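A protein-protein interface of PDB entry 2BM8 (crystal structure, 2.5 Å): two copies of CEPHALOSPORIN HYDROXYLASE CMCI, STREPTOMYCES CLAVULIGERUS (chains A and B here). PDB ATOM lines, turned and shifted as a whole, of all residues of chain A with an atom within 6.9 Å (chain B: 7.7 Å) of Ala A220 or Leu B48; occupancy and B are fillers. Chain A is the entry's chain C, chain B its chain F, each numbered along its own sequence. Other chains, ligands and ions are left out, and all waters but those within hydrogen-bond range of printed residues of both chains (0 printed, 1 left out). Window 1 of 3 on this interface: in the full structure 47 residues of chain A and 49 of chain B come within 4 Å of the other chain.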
ATOM      1  N   ASP A  68     -30.033 -20.807   3.298  1.00  0.00           N
ATOM      2  CA  ASP A  68     -29.898 -19.376   3.015  1.00  0.00           C
ATOM      3  C   ASP A  68     -31.045 -18.846   2.132  1.00  0.00           C
ATOM      4  O   ASP A  68     -31.460 -17.707   2.288  1.00  0.00           O
ATOM      5  CB  ASP A  68     -28.502 -18.891   2.544  1.00  0.00           C
ATOM      6  CG  ASP A  68     -27.702 -19.927   1.845  1.00  0.00           C
ATOM      7  OD1 ASP A  68     -27.978 -20.149   0.628  1.00  0.00           O
ATOM      8  OD2 ASP A  68     -26.746 -20.530   2.418  1.00  0.00           O
ATOM      9  N   THR A  69     -31.566 -19.674   1.241  1.00  0.00           N
ATOM     10  CA  THR A  69     -32.742 -19.320   0.480  1.00  0.00           C
ATOM     11  C   THR A  69     -33.939 -19.083   1.428  1.00  0.00           C
ATOM     12  O   THR A  69     -34.669 -18.099   1.287  1.00  0.00           O
ATOM     13  CB  THR A  69     -33.021 -20.431  -0.542  1.00  0.00           C
ATOM     14  OG1 THR A  69     -31.915 -20.512  -1.457  1.00  0.00           O
ATOM     15  CG2 THR A  69     -34.206 -20.093  -1.435  1.00  0.00           C
ATOM     16  N   ALA A  71     -33.884 -18.121   4.511  1.00  0.00           N
ATOM     17  CA  ALA A  71     -33.666 -16.889   5.255  1.00  0.00           C
ATOM     18  C   ALA A  71     -34.068 -15.684   4.418  1.00  0.00           C
ATOM     19  O   ALA A  71     -34.730 -14.792   4.930  1.00  0.00           O
ATOM     20  CB  ALA A  71     -32.219 -16.775   5.679  1.00  0.00           C
ATOM     21  N   VAL A  72     -33.675 -15.669   3.138  1.00  0.00           N
ATOM     22  CA  VAL A  72     -34.078 -14.621   2.194  1.00  0.00           C
ATOM     23  C   VAL A  72     -35.600 -14.483   2.107  1.00  0.00           C
ATOM     24  O   VAL A  72     -36.125 -13.373   2.096  1.00  0.00           O
ATOM     25  CB  VAL A  72     -33.543 -14.890   0.764  1.00  0.00           C
ATOM     26  CG1 VAL A  72     -34.129 -13.892  -0.235  1.00  0.00           C
ATOM     27  CG2 VAL A  72     -32.001 -14.848   0.717  1.00  0.00           C
ATOM     28  N   MET A 215     -31.820  -5.871  -5.520  1.00  0.00           N
ATOM     29  CA  MET A 215     -30.447  -6.106  -5.069  1.00  0.00           C
ATOM     30  C   MET A 215     -30.328  -6.361  -3.560  1.00  0.00           C
ATOM     31  O   MET A 215     -29.280  -6.809  -3.102  1.00  0.00           O
ATOM     32  CB  MET A 215     -29.537  -4.934  -5.468  1.00  0.00           C
ATOM     33  CG  MET A 215     -29.473  -4.637  -6.972  1.00  0.00           C
ATOM     34  SD  MET A 215     -28.865  -6.027  -7.946  1.00  0.00           S
ATOM     35  CE  MET A 215     -27.214  -6.193  -7.313  1.00  0.00           C
ATOM     36  N   LEU A 216     -31.386  -6.080  -2.793  1.00  0.00           N
ATOM     37  CA  LEU A 216     -31.430  -6.470  -1.378  1.00  0.00           C
ATOM     38  C   LEU A 216     -31.405  -7.978  -1.193  1.00  0.00           C
ATOM     39  O   LEU A 216     -30.831  -8.463  -0.230  1.00  0.00           O
ATOM     40  CB  LEU A 216     -32.670  -5.905  -0.674  1.00  0.00           C
ATOM     41  CG  LEU A 216     -32.667  -6.014   0.865  1.00  0.00           C
ATOM     42  CD1 LEU A 216     -31.487  -5.269   1.452  1.00  0.00           C
ATOM     43  CD2 LEU A 216     -33.957  -5.476   1.490  1.00  0.00           C
ATOM     44  N   TYR A 217     -32.033  -8.710  -2.108  1.00  0.00           N
ATOM     45  CA  TYR A 217     -32.143 -10.171  -2.009  1.00  0.00           C
ATOM     46  C   TYR A 217     -31.441 -10.956  -3.113  1.00  0.00           C
ATOM     47  O   TYR A 217     -31.154 -12.128  -2.940  1.00  0.00           O
ATOM     48  CB  TYR A 217     -33.618 -10.553  -2.018  1.00  0.00           C
ATOM     49  CG  TYR A 217     -34.396  -9.904  -0.901  1.00  0.00           C
ATOM     50  CD1 TYR A 217     -35.588  -9.237  -1.149  1.00  0.00           C
ATOM     51  CD2 TYR A 217     -33.918  -9.950   0.422  1.00  0.00           C
ATOM     52  CE1 TYR A 217     -36.300  -8.642  -0.109  1.00  0.00           C
ATOM     53  CE2 TYR A 217     -34.616  -9.360   1.459  1.00  0.00           C
ATOM     54  CZ  TYR A 217     -35.802  -8.704   1.194  1.00  0.00           C
ATOM     55  OH  TYR A 217     -36.474  -8.118   2.239  1.00  0.00           O
ATOM     56  N   ALA A 218     -31.147 -10.320  -4.237  1.00  0.00           N
ATOM     57  CA  ALA A 218     -30.729 -11.030  -5.447  1.00  0.00           C
ATOM     58  C   ALA A 218     -29.352 -11.667  -5.336  1.00  0.00           C
ATOM     59  O   ALA A 218     -29.032 -12.570  -6.103  1.00  0.00           O
ATOM     60  CB  ALA A 218     -30.764 -10.069  -6.669  1.00  0.00           C
ATOM     61  N   ASN A 219     -28.525 -11.170  -4.417  1.00  0.00           N
ATOM     62  CA  ASN A 219     -27.202 -11.751  -4.170  1.00  0.00           C
ATOM     63  C   ASN A 219     -27.119 -12.472  -2.828  1.00  0.00           C
ATOM     64  O   ASN A 219     -26.036 -12.790  -2.376  1.00  0.00           O
ATOM     65  CB  ASN A 219     -26.125 -10.659  -4.226  1.00  0.00           C
ATOM     66  CG  ASN A 219     -25.978 -10.044  -5.613  1.00  0.00           C
ATOM     67  OD1 ASN A 219     -25.872 -10.755  -6.612  1.00  0.00           O
ATOM     68  ND2 ASN A 219     -25.961  -8.721  -5.673  1.00  0.00           N
ATOM     69  N   ALA A 220     -28.258 -12.762  -2.202  1.00  0.00           N
ATOM     70  CA  ALA A 220     -28.273 -13.253  -0.811  1.00  0.00           C
ATOM     71  C   ALA A 220     -28.304 -14.770  -0.681  1.00  0.00           C
ATOM     72  O   ALA A 220     -28.187 -15.291   0.420  1.00  0.00           O
ATOM     73  CB  ALA A 220     -29.436 -12.639  -0.040  1.00  0.00           C
ATOM     74  N   SER A 221     -28.482 -15.478  -1.788  1.00  0.00           N
ATOM     75  CA  SER A 221     -28.371 -16.926  -1.778  1.00  0.00           C
ATOM     76  C   SER A 221     -28.056 -17.467  -3.170  1.00  0.00           C
ATOM     77  O   SER A 221     -28.414 -16.858  -4.180  1.00  0.00           O
ATOM     78  CB  SER A 221     -29.649 -17.557  -1.214  1.00  0.00           C
ATOM     79  OG  SER A 221     -30.489 -18.063  -2.234  1.00  0.00           O
ATOM     80  N   SER A 222     -27.388 -18.621  -3.211  1.00  0.00           N
ATOM     81  CA  SER A 222     -26.970 -19.224  -4.470  1.00  0.00           C
ATOM     82  C   SER A 222     -28.160 -19.689  -5.323  1.00  0.00           C
ATOM     83  O   SER A 222     -28.073 -19.702  -6.544  1.00  0.00           O
ATOM     84  CB  SER A 222     -25.999 -20.379  -4.217  1.00  0.00           C
ATOM     85  OG  SER A 222     -26.683 -21.524  -3.736  1.00  0.00           O
ATOM     86  N   GLN A 223     -29.271 -20.049  -4.694  1.00  0.00           N
ATOM     87  CA  GLN A 223     -30.466 -20.448  -5.445  1.00  0.00           C
ATOM     88  C   GLN A 223     -31.238 -19.247  -6.019  1.00  0.00           C
ATOM     89  O   GLN A 223     -31.873 -19.361  -7.051  1.00  0.00           O
ATOM     90  CB  GLN A 223     -31.409 -21.314  -4.595  1.00  0.00           C
ATOM     91  CG  GLN A 223     -30.930 -22.748  -4.353  1.00  0.00           C
ATOM     92  CD  GLN A 223     -31.836 -23.511  -3.381  1.00  0.00           C
ATOM     93  OE1 GLN A 223     -32.364 -22.924  -2.421  1.00  0.00           O
ATOM     94  NE2 GLN A 223     -32.026 -24.809  -3.630  1.00  0.00           N
ATOM     95  N   LEU A 224     -31.184 -18.102  -5.361  1.00  0.00           N
ATOM     96  CA  LEU A 224     -31.944 -16.943  -5.817  1.00  0.00           C
ATOM     97  C   LEU A 224     -31.081 -16.010  -6.638  1.00  0.00           C
ATOM     98  O   LEU A 224     -31.574 -15.043  -7.189  1.00  0.00           O
ATOM     99  CB  LEU A 224     -32.535 -16.194  -4.628  1.00  0.00           C
ATOM    100  CG  LEU A 224     -33.566 -16.970  -3.816  1.00  0.00           C
ATOM    101  CD1 LEU A 224     -34.046 -16.082  -2.692  1.00  0.00           C
ATOM    102  CD2 LEU A 224     -34.726 -17.436  -4.658  1.00  0.00           C
ATOM    103  N   ASP A 225     -29.794 -16.344  -6.714  1.00  0.00           N
ATOM    104  CA  ASP A 225     -28.769 -15.606  -7.447  1.00  0.00           C
ATOM    105  C   ASP A 225     -29.234 -14.867  -8.717  1.00  0.00           C
ATOM    106  O   ASP A 225     -29.610 -15.486  -9.706  1.00  0.00           O
ATOM    107  CB  ASP A 225     -27.653 -16.598  -7.802  1.00  0.00           C
ATOM    108  CG  ASP A 225     -26.438 -15.934  -8.403  1.00  0.00           C
ATOM    109  OD1 ASP A 225     -26.314 -14.695  -8.364  1.00  0.00           O
ATOM    110  OD2 ASP A 225     -25.544 -16.605  -8.939  1.00  0.00           O
ATOM    111  N   ARG A 226     -29.123 -13.542  -8.678  1.00  0.00           N
ATOM    112  CA  ARG A 226     -29.660 -12.609  -9.681  1.00  0.00           C
ATOM    113  C   ARG A 226     -30.912 -13.055 -10.438  1.00  0.00           C
ATOM    114  O   ARG A 226     -30.977 -12.958 -11.661  1.00  0.00           O
ATOM    115  CB  ARG A 226     -28.572 -12.105 -10.648  1.00  0.00           C
ATOM    116  CG  ARG A 226     -27.567 -13.102 -11.128  1.00  0.00           C
ATOM    117  CD  ARG A 226     -26.135 -12.748 -10.780  1.00  0.00           C
ATOM    118  NE  ARG A 226     -25.321 -13.966 -10.749  1.00  0.00           N
ATOM    119  CZ  ARG A 226     -24.850 -14.596 -11.827  1.00  0.00           C
ATOM    120  NH1 ARG A 226     -25.067 -14.121 -13.054  1.00  0.00           N
ATOM    121  NH2 ARG A 226     -24.135 -15.704 -11.670  1.00  0.00           N
ATOM    122  N   PRO B  27     -30.821  -4.922   6.782  1.00  0.00           N
ATOM    123  CA  PRO B  27     -29.715  -4.398   5.978  1.00  0.00           C
ATOM    124  C   PRO B  27     -30.140  -3.246   5.060  1.00  0.00           C
ATOM    125  O   PRO B  27     -31.304  -3.177   4.648  1.00  0.00           O
ATOM    126  CB  PRO B  27     -29.305  -5.598   5.123  1.00  0.00           C
ATOM    127  CG  PRO B  27     -29.785  -6.810   5.859  1.00  0.00           C
ATOM    128  CD  PRO B  27     -30.960  -6.384   6.664  1.00  0.00           C
ATOM    129  N   LEU B  29     -28.647  -1.155   1.469  1.00  0.00           N
ATOM    130  CA  LEU B  29     -27.679  -0.951   0.400  1.00  0.00           C
ATOM    131  C   LEU B  29     -27.183   0.489   0.470  1.00  0.00           C
ATOM    132  O   LEU B  29     -27.988   1.427   0.610  1.00  0.00           O
ATOM    133  CB  LEU B  29     -28.308  -1.225  -0.973  1.00  0.00           C
ATOM    134  CG  LEU B  29     -28.405  -2.664  -1.515  1.00  0.00           C
ATOM    135  CD1 LEU B  29     -27.718  -3.701  -0.631  1.00  0.00           C
ATOM    136  CD2 LEU B  29     -29.854  -3.042  -1.755  1.00  0.00           C
ATOM    137  N   ASP B  31     -24.151   1.396  -1.731  1.00  0.00           N
ATOM    138  CA  ASP B  31     -23.345   1.652  -2.928  1.00  0.00           C
ATOM    139  C   ASP B  31     -24.002   1.213  -4.251  1.00  0.00           C
ATOM    140  O   ASP B  31     -23.345   1.214  -5.299  1.00  0.00           O
ATOM    141  CB  ASP B  31     -21.961   1.006  -2.775  1.00  0.00           C
ATOM    142  CG  ASP B  31     -21.972  -0.491  -3.057  1.00  0.00           C
ATOM    143  OD1 ASP B  31     -22.948  -1.185  -2.676  1.00  0.00           O
ATOM    144  OD2 ASP B  31     -21.041  -1.063  -3.662  1.00  0.00           O
ATOM    145  N   ARG B  32     -25.277   0.817  -4.206  1.00  0.00           N
ATOM    146  CA  ARG B  32     -26.059   0.622  -5.436  1.00  0.00           C
ATOM    147  C   ARG B  32     -27.540   0.874  -5.213  1.00  0.00           C
ATOM    148  O   ARG B  32     -28.006   0.899  -4.078  1.00  0.00           O
ATOM    149  CB  ARG B  32     -25.878  -0.778  -6.038  1.00  0.00           C
ATOM    150  CG  ARG B  32     -24.977  -1.727  -5.284  1.00  0.00           C
ATOM    151  CD  ARG B  32     -25.620  -2.424  -4.110  1.00  0.00           C
ATOM    152  NE  ARG B  32     -25.412  -3.872  -4.181  1.00  0.00           N
ATOM    153  CZ  ARG B  32     -24.238  -4.497  -4.072  1.00  0.00           C
ATOM    154  NH1 ARG B  32     -23.109  -3.825  -3.886  1.00  0.00           N
ATOM    155  NH2 ARG B  32     -24.191  -5.816  -4.158  1.00  0.00           N
ATOM    156  N   PRO B  45     -23.432  -5.612  -9.527  1.00  0.00           N
ATOM    157  CA  PRO B  45     -22.437  -6.129  -8.591  1.00  0.00           C
ATOM    158  C   PRO B  45     -22.935  -7.439  -7.973  1.00  0.00           C
ATOM    159  O   PRO B  45     -24.134  -7.610  -7.712  1.00  0.00           O
ATOM    160  CB  PRO B  45     -22.283  -5.002  -7.571  1.00  0.00           C
ATOM    161  CG  PRO B  45     -23.533  -4.219  -7.658  1.00  0.00           C
ATOM    162  CD  PRO B  45     -24.072  -4.376  -9.037  1.00  0.00           C
ATOM    163  N   ARG B  46     -22.000  -8.359  -7.784  1.00  0.00           N
ATOM    164  CA  ARG B  46     -22.314  -9.749  -7.492  1.00  0.00           C
ATOM    165  C   ARG B  46     -22.149 -10.098  -6.029  1.00  0.00           C
ATOM    166  O   ARG B  46     -22.532 -11.185  -5.625  1.00  0.00           O
ATOM    167  CB  ARG B  46     -21.410 -10.655  -8.321  1.00  0.00           C
ATOM    168  CG  ARG B  46     -21.665 -10.544  -9.815  1.00  0.00           C
ATOM    169  CD  ARG B  46     -22.713 -11.514 -10.317  1.00  0.00           C
ATOM    170  NE  ARG B  46     -22.441 -12.855  -9.815  1.00  0.00           N
ATOM    171  CZ  ARG B  46     -21.498 -13.668 -10.280  1.00  0.00           C
ATOM    172  NH1 ARG B  46     -20.719 -13.314 -11.292  1.00  0.00           N
ATOM    173  NH2 ARG B  46     -21.338 -14.857  -9.728  1.00  0.00           N
ATOM    174  N   ASP B  47     -21.558  -9.196  -5.253  1.00  0.00           N
ATOM    175  CA  ASP B  47     -21.401  -9.394  -3.814  1.00  0.00           C
ATOM    176  C   ASP B  47     -22.669  -9.013  -3.049  1.00  0.00           C
ATOM    177  O   ASP B  47     -23.546  -8.335  -3.571  1.00  0.00           O
ATOM    178  CB  ASP B  47     -20.181  -8.626  -3.282  1.00  0.00           C
ATOM    179  CG  ASP B  47     -20.385  -7.122  -3.262  1.00  0.00           C
ATOM    180  OD1 ASP B  47     -19.886  -6.482  -2.316  1.00  0.00           O
ATOM    181  OD2 ASP B  47     -21.008  -6.487  -4.139  1.00  0.00           O
ATOM    182  N   LEU B  48     -22.744  -9.453  -1.802  1.00  0.00           N
ATOM    183  CA  LEU B  48     -23.956  -9.327  -0.992  1.00  0.00           C
ATOM    184  C   LEU B  48     -24.527  -7.916  -1.001  1.00  0.00           C
ATOM    185  O   LEU B  48     -25.705  -7.729  -1.297  1.00  0.00           O
ATOM    186  CB  LEU B  48     -23.670  -9.776   0.445  1.00  0.00           C
ATOM    187  CG  LEU B  48     -24.796 -10.273   1.358  1.00  0.00           C
ATOM    188  CD1 LEU B  48     -25.761 -11.230   0.670  1.00  0.00           C
ATOM    189  CD2 LEU B  48     -24.166 -10.947   2.579  1.00  0.00           C
ATOM    190  N   GLY B  49     -23.693  -6.930  -0.690  1.00  0.00           N
ATOM    191  CA  GLY B  49     -24.128  -5.544  -0.609  1.00  0.00           C
ATOM    192  C   GLY B  49     -23.995  -4.928   0.774  1.00  0.00           C
ATOM    193  O   GLY B  49     -24.094  -3.713   0.919  1.00  0.00           O
ATOM    194  N   TYR B  50     -23.769  -5.762   1.789  1.00  0.00           N
ATOM    195  CA  TYR B  50     -23.694  -5.304   3.180  1.00  0.00           C
ATOM    196  C   TYR B  50     -22.914  -6.290   4.068  1.00  0.00           C
ATOM    197  O   TYR B  50     -22.453  -7.331   3.592  1.00  0.00           O
ATOM    198  CB  TYR B  50     -25.115  -5.082   3.725  1.00  0.00           C
ATOM    199  CG  TYR B  50     -26.077  -6.247   3.503  1.00  0.00           C
ATOM    200  CD1 TYR B  50     -26.192  -7.267   4.444  1.00  0.00           C
ATOM    201  CD2 TYR B  50     -26.891  -6.315   2.368  1.00  0.00           C
ATOM    202  CE1 TYR B  50     -27.071  -8.331   4.262  1.00  0.00           C
ATOM    203  CE2 TYR B  50     -27.783  -7.381   2.183  1.00  0.00           C
ATOM    204  CZ  TYR B  50     -27.858  -8.386   3.139  1.00  0.00           C
ATOM    205  OH  TYR B  50     -28.711  -9.447   2.982  1.00  0.00           O
ATOM    206  N   SER B  51     -22.746  -5.959   5.348  1.00  0.00           N
ATOM    207  CA  SER B  51     -22.049  -6.856   6.285  1.00  0.00           C
ATOM    208  C   SER B  51     -22.727  -8.248   6.374  1.00  0.00           C
ATOM    209  O   SER B  51     -23.952  -8.331   6.425  1.00  0.00           O
ATOM    210  CB  SER B  51     -21.996  -6.219   7.679  1.00  0.00           C
ATOM    211  OG  SER B  51     -23.302  -5.916   8.153  1.00  0.00           O
ATOM    212  N   ASP B  52     -21.937  -9.328   6.393  1.00  0.00           N
ATOM    213  CA  ASP B  52     -22.491 -10.689   6.568  1.00  0.00           C
ATOM    214  C   ASP B  52     -22.303 -11.249   7.997  1.00  0.00           C
ATOM    215  O   ASP B  52     -22.445 -12.466   8.222  1.00  0.00           O
ATOM    216  CB  ASP B  52     -21.922 -11.673   5.514  1.00  0.00           C
ATOM    217  CG  ASP B  52     -20.480 -12.105   5.801  1.00  0.00           C
ATOM    218  OD1 ASP B  52     -19.997 -13.028   5.109  1.00  0.00           O
ATOM    219  OD2 ASP B  52     -19.763 -11.598   6.690  1.00  0.00           O
ATOM    220  N   PHE B  53     -22.014 -10.358   8.954  1.00  0.00           N
ATOM    221  CA  PHE B  53     -21.674 -10.761  10.320  1.00  0.00           C
ATOM    222  C   PHE B  53     -22.806 -11.573  10.953  1.00  0.00           C
ATOM    223  O   PHE B  53     -22.632 -12.771  11.193  1.00  0.00           O
ATOM    224  CB  PHE B  53     -21.308  -9.552  11.215  1.00  0.00           C
ATOM    225  CG  PHE B  53     -21.649  -9.758  12.673  1.00  0.00           C
ATOM    226  CD1 PHE B  53     -21.141 -10.871  13.369  1.00  0.00           C
ATOM    227  CD2 PHE B  53     -22.517  -8.886  13.334  1.00  0.00           C
ATOM    228  CE1 PHE B  53     -21.471 -11.087  14.694  1.00  0.00           C
ATOM    229  CE2 PHE B  53     -22.844  -9.098  14.665  1.00  0.00           C
ATOM    230  CZ  PHE B  53     -22.321 -10.191  15.348  1.00  0.00           C
ATOM    231  N   PRO B  55     -26.656 -10.905  10.033  1.00  0.00           N
ATOM    232  CA  PRO B  55     -27.766 -10.147   9.463  1.00  0.00           C
ATOM    233  C   PRO B  55     -29.058 -10.952   9.461  1.00  0.00           C
ATOM    234  O   PRO B  55     -29.820 -10.857   8.520  1.00  0.00           O
ATOM    235  CB  PRO B  55     -27.289  -9.926   8.032  1.00  0.00           C
ATOM    236  CG  PRO B  55     -26.559 -11.215   7.712  1.00  0.00           C
ATOM    237  CD  PRO B  55     -25.950 -11.683   8.995  1.00  0.00           C
ATOM    238  N   TYR B  56     -29.296 -11.744  10.497  1.00  0.00           N
ATOM    239  CA  TYR B  56     -30.374 -12.722  10.470  1.00  0.00           C
ATOM    240  C   TYR B  56     -31.473 -12.355  11.454  1.00  0.00           C
ATOM    241  O   TYR B  56     -31.240 -11.639  12.419  1.00  0.00           O
ATOM    242  CB  TYR B  56     -29.812 -14.116  10.751  1.00  0.00           C
ATOM    243  CG  TYR B  56     -28.808 -14.594   9.714  1.00  0.00           C
ATOM    244  CD1 TYR B  56     -27.477 -14.843  10.051  1.00  0.00           C
ATOM    245  CD2 TYR B  56     -29.200 -14.820   8.396  1.00  0.00           C
ATOM    246  CE1 TYR B  56     -26.564 -15.291   9.092  1.00  0.00           C
ATOM    247  CE2 TYR B  56     -28.306 -15.264   7.434  1.00  0.00           C
ATOM    248  CZ  TYR B  56     -26.990 -15.495   7.778  1.00  0.00           C
ATOM    249  OH  TYR B  56     -26.114 -15.935   6.799  1.00  0.00           O
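Hydrophobic or aromatic side chains of chain A that line the printed part of chain B: Met A215, Leu A216 and Ala A220. Hydrophobic or aromatic side chains of chain B within 4 Å of the printed part of chain A: Leu B29, Leu B48 and Tyr B50. Among the printed residues, no Asp or Glu carboxylate lies within 4 Å of a Lys or Arg side-chain nitrogen of the other chain.
No position is printed for both chains. Of the 12 pairs that touch across the chains among the printed residues, none has its exchanged pair printed and touching as well.
Among the printed residues, pairs that only touch across the chains: Met A215 with Leu B29, Met A215 with Pro B45, Leu A216 with Pro B27, Leu A216 with Leu B29, Leu A216 with Tyr B50, Asn A219 with Arg B32, Asn A219 with Arg B46, Asn A219 with Leu B48 and Ala A220 with Leu B48.
NE of Arg A226 sits close to NE of Arg B46. The side-chain amide nitrogen of Asn A219 is in hydrogen-bond range of the backbone carbonyl oxygen of Pro B45. The side-chain amide nitrogen of Asn A219 lies within hydrogen-bond range of the backbone carbonyl oxygen of Asp B47 (3.2 Å).
OD1 of Asp B31 lies within salt-bridge range of NH1 of Arg B32 (2.9 Å). OD1 of Asp A225 is in salt-bridge range of NE of Arg A226. The guanidinium group (NH2) of Arg B32 is in salt-bridge range of the side-chain carboxylate (OD2) of Asp B47 (3.3 Å). The backbone carbonyl oxygen (O) of Ala A218 sits at hydrogen-bond distance from the backbone NH (N) of Arg A226 (2.8 Å).
Of the printed residues of chain B, Asn A219 touches Arg B32, Pro B45, Arg B46, Asp B47 and Leu B48. Ala A220 touches just one residue of chain B: Leu B48 (3.5 Å). Of the printed residues of chain B, Arg A226 touches Arg B46 (3.2 Å). Printed residues of chain A within 4 Å of Arg B32: Asn A219 (3.7 Å). Of the printed residues of chain A, Arg B46 touches Asn A219 and Arg A226. Leu B48 touches just these residues of chain A: Asn A219 (3.4 Å) and Ala A220 (3.5 Å). Gly B49 touches none of the printed residues of chain A. Pro B55 touches none of the printed residues of chain A. The nearest residue of chain B that does not touch Ala A220 is Tyr B50 (4.5 Å). The nearest printed residue of chain A that does not touch Pro B45 is Arg A226 (6.3 Å).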
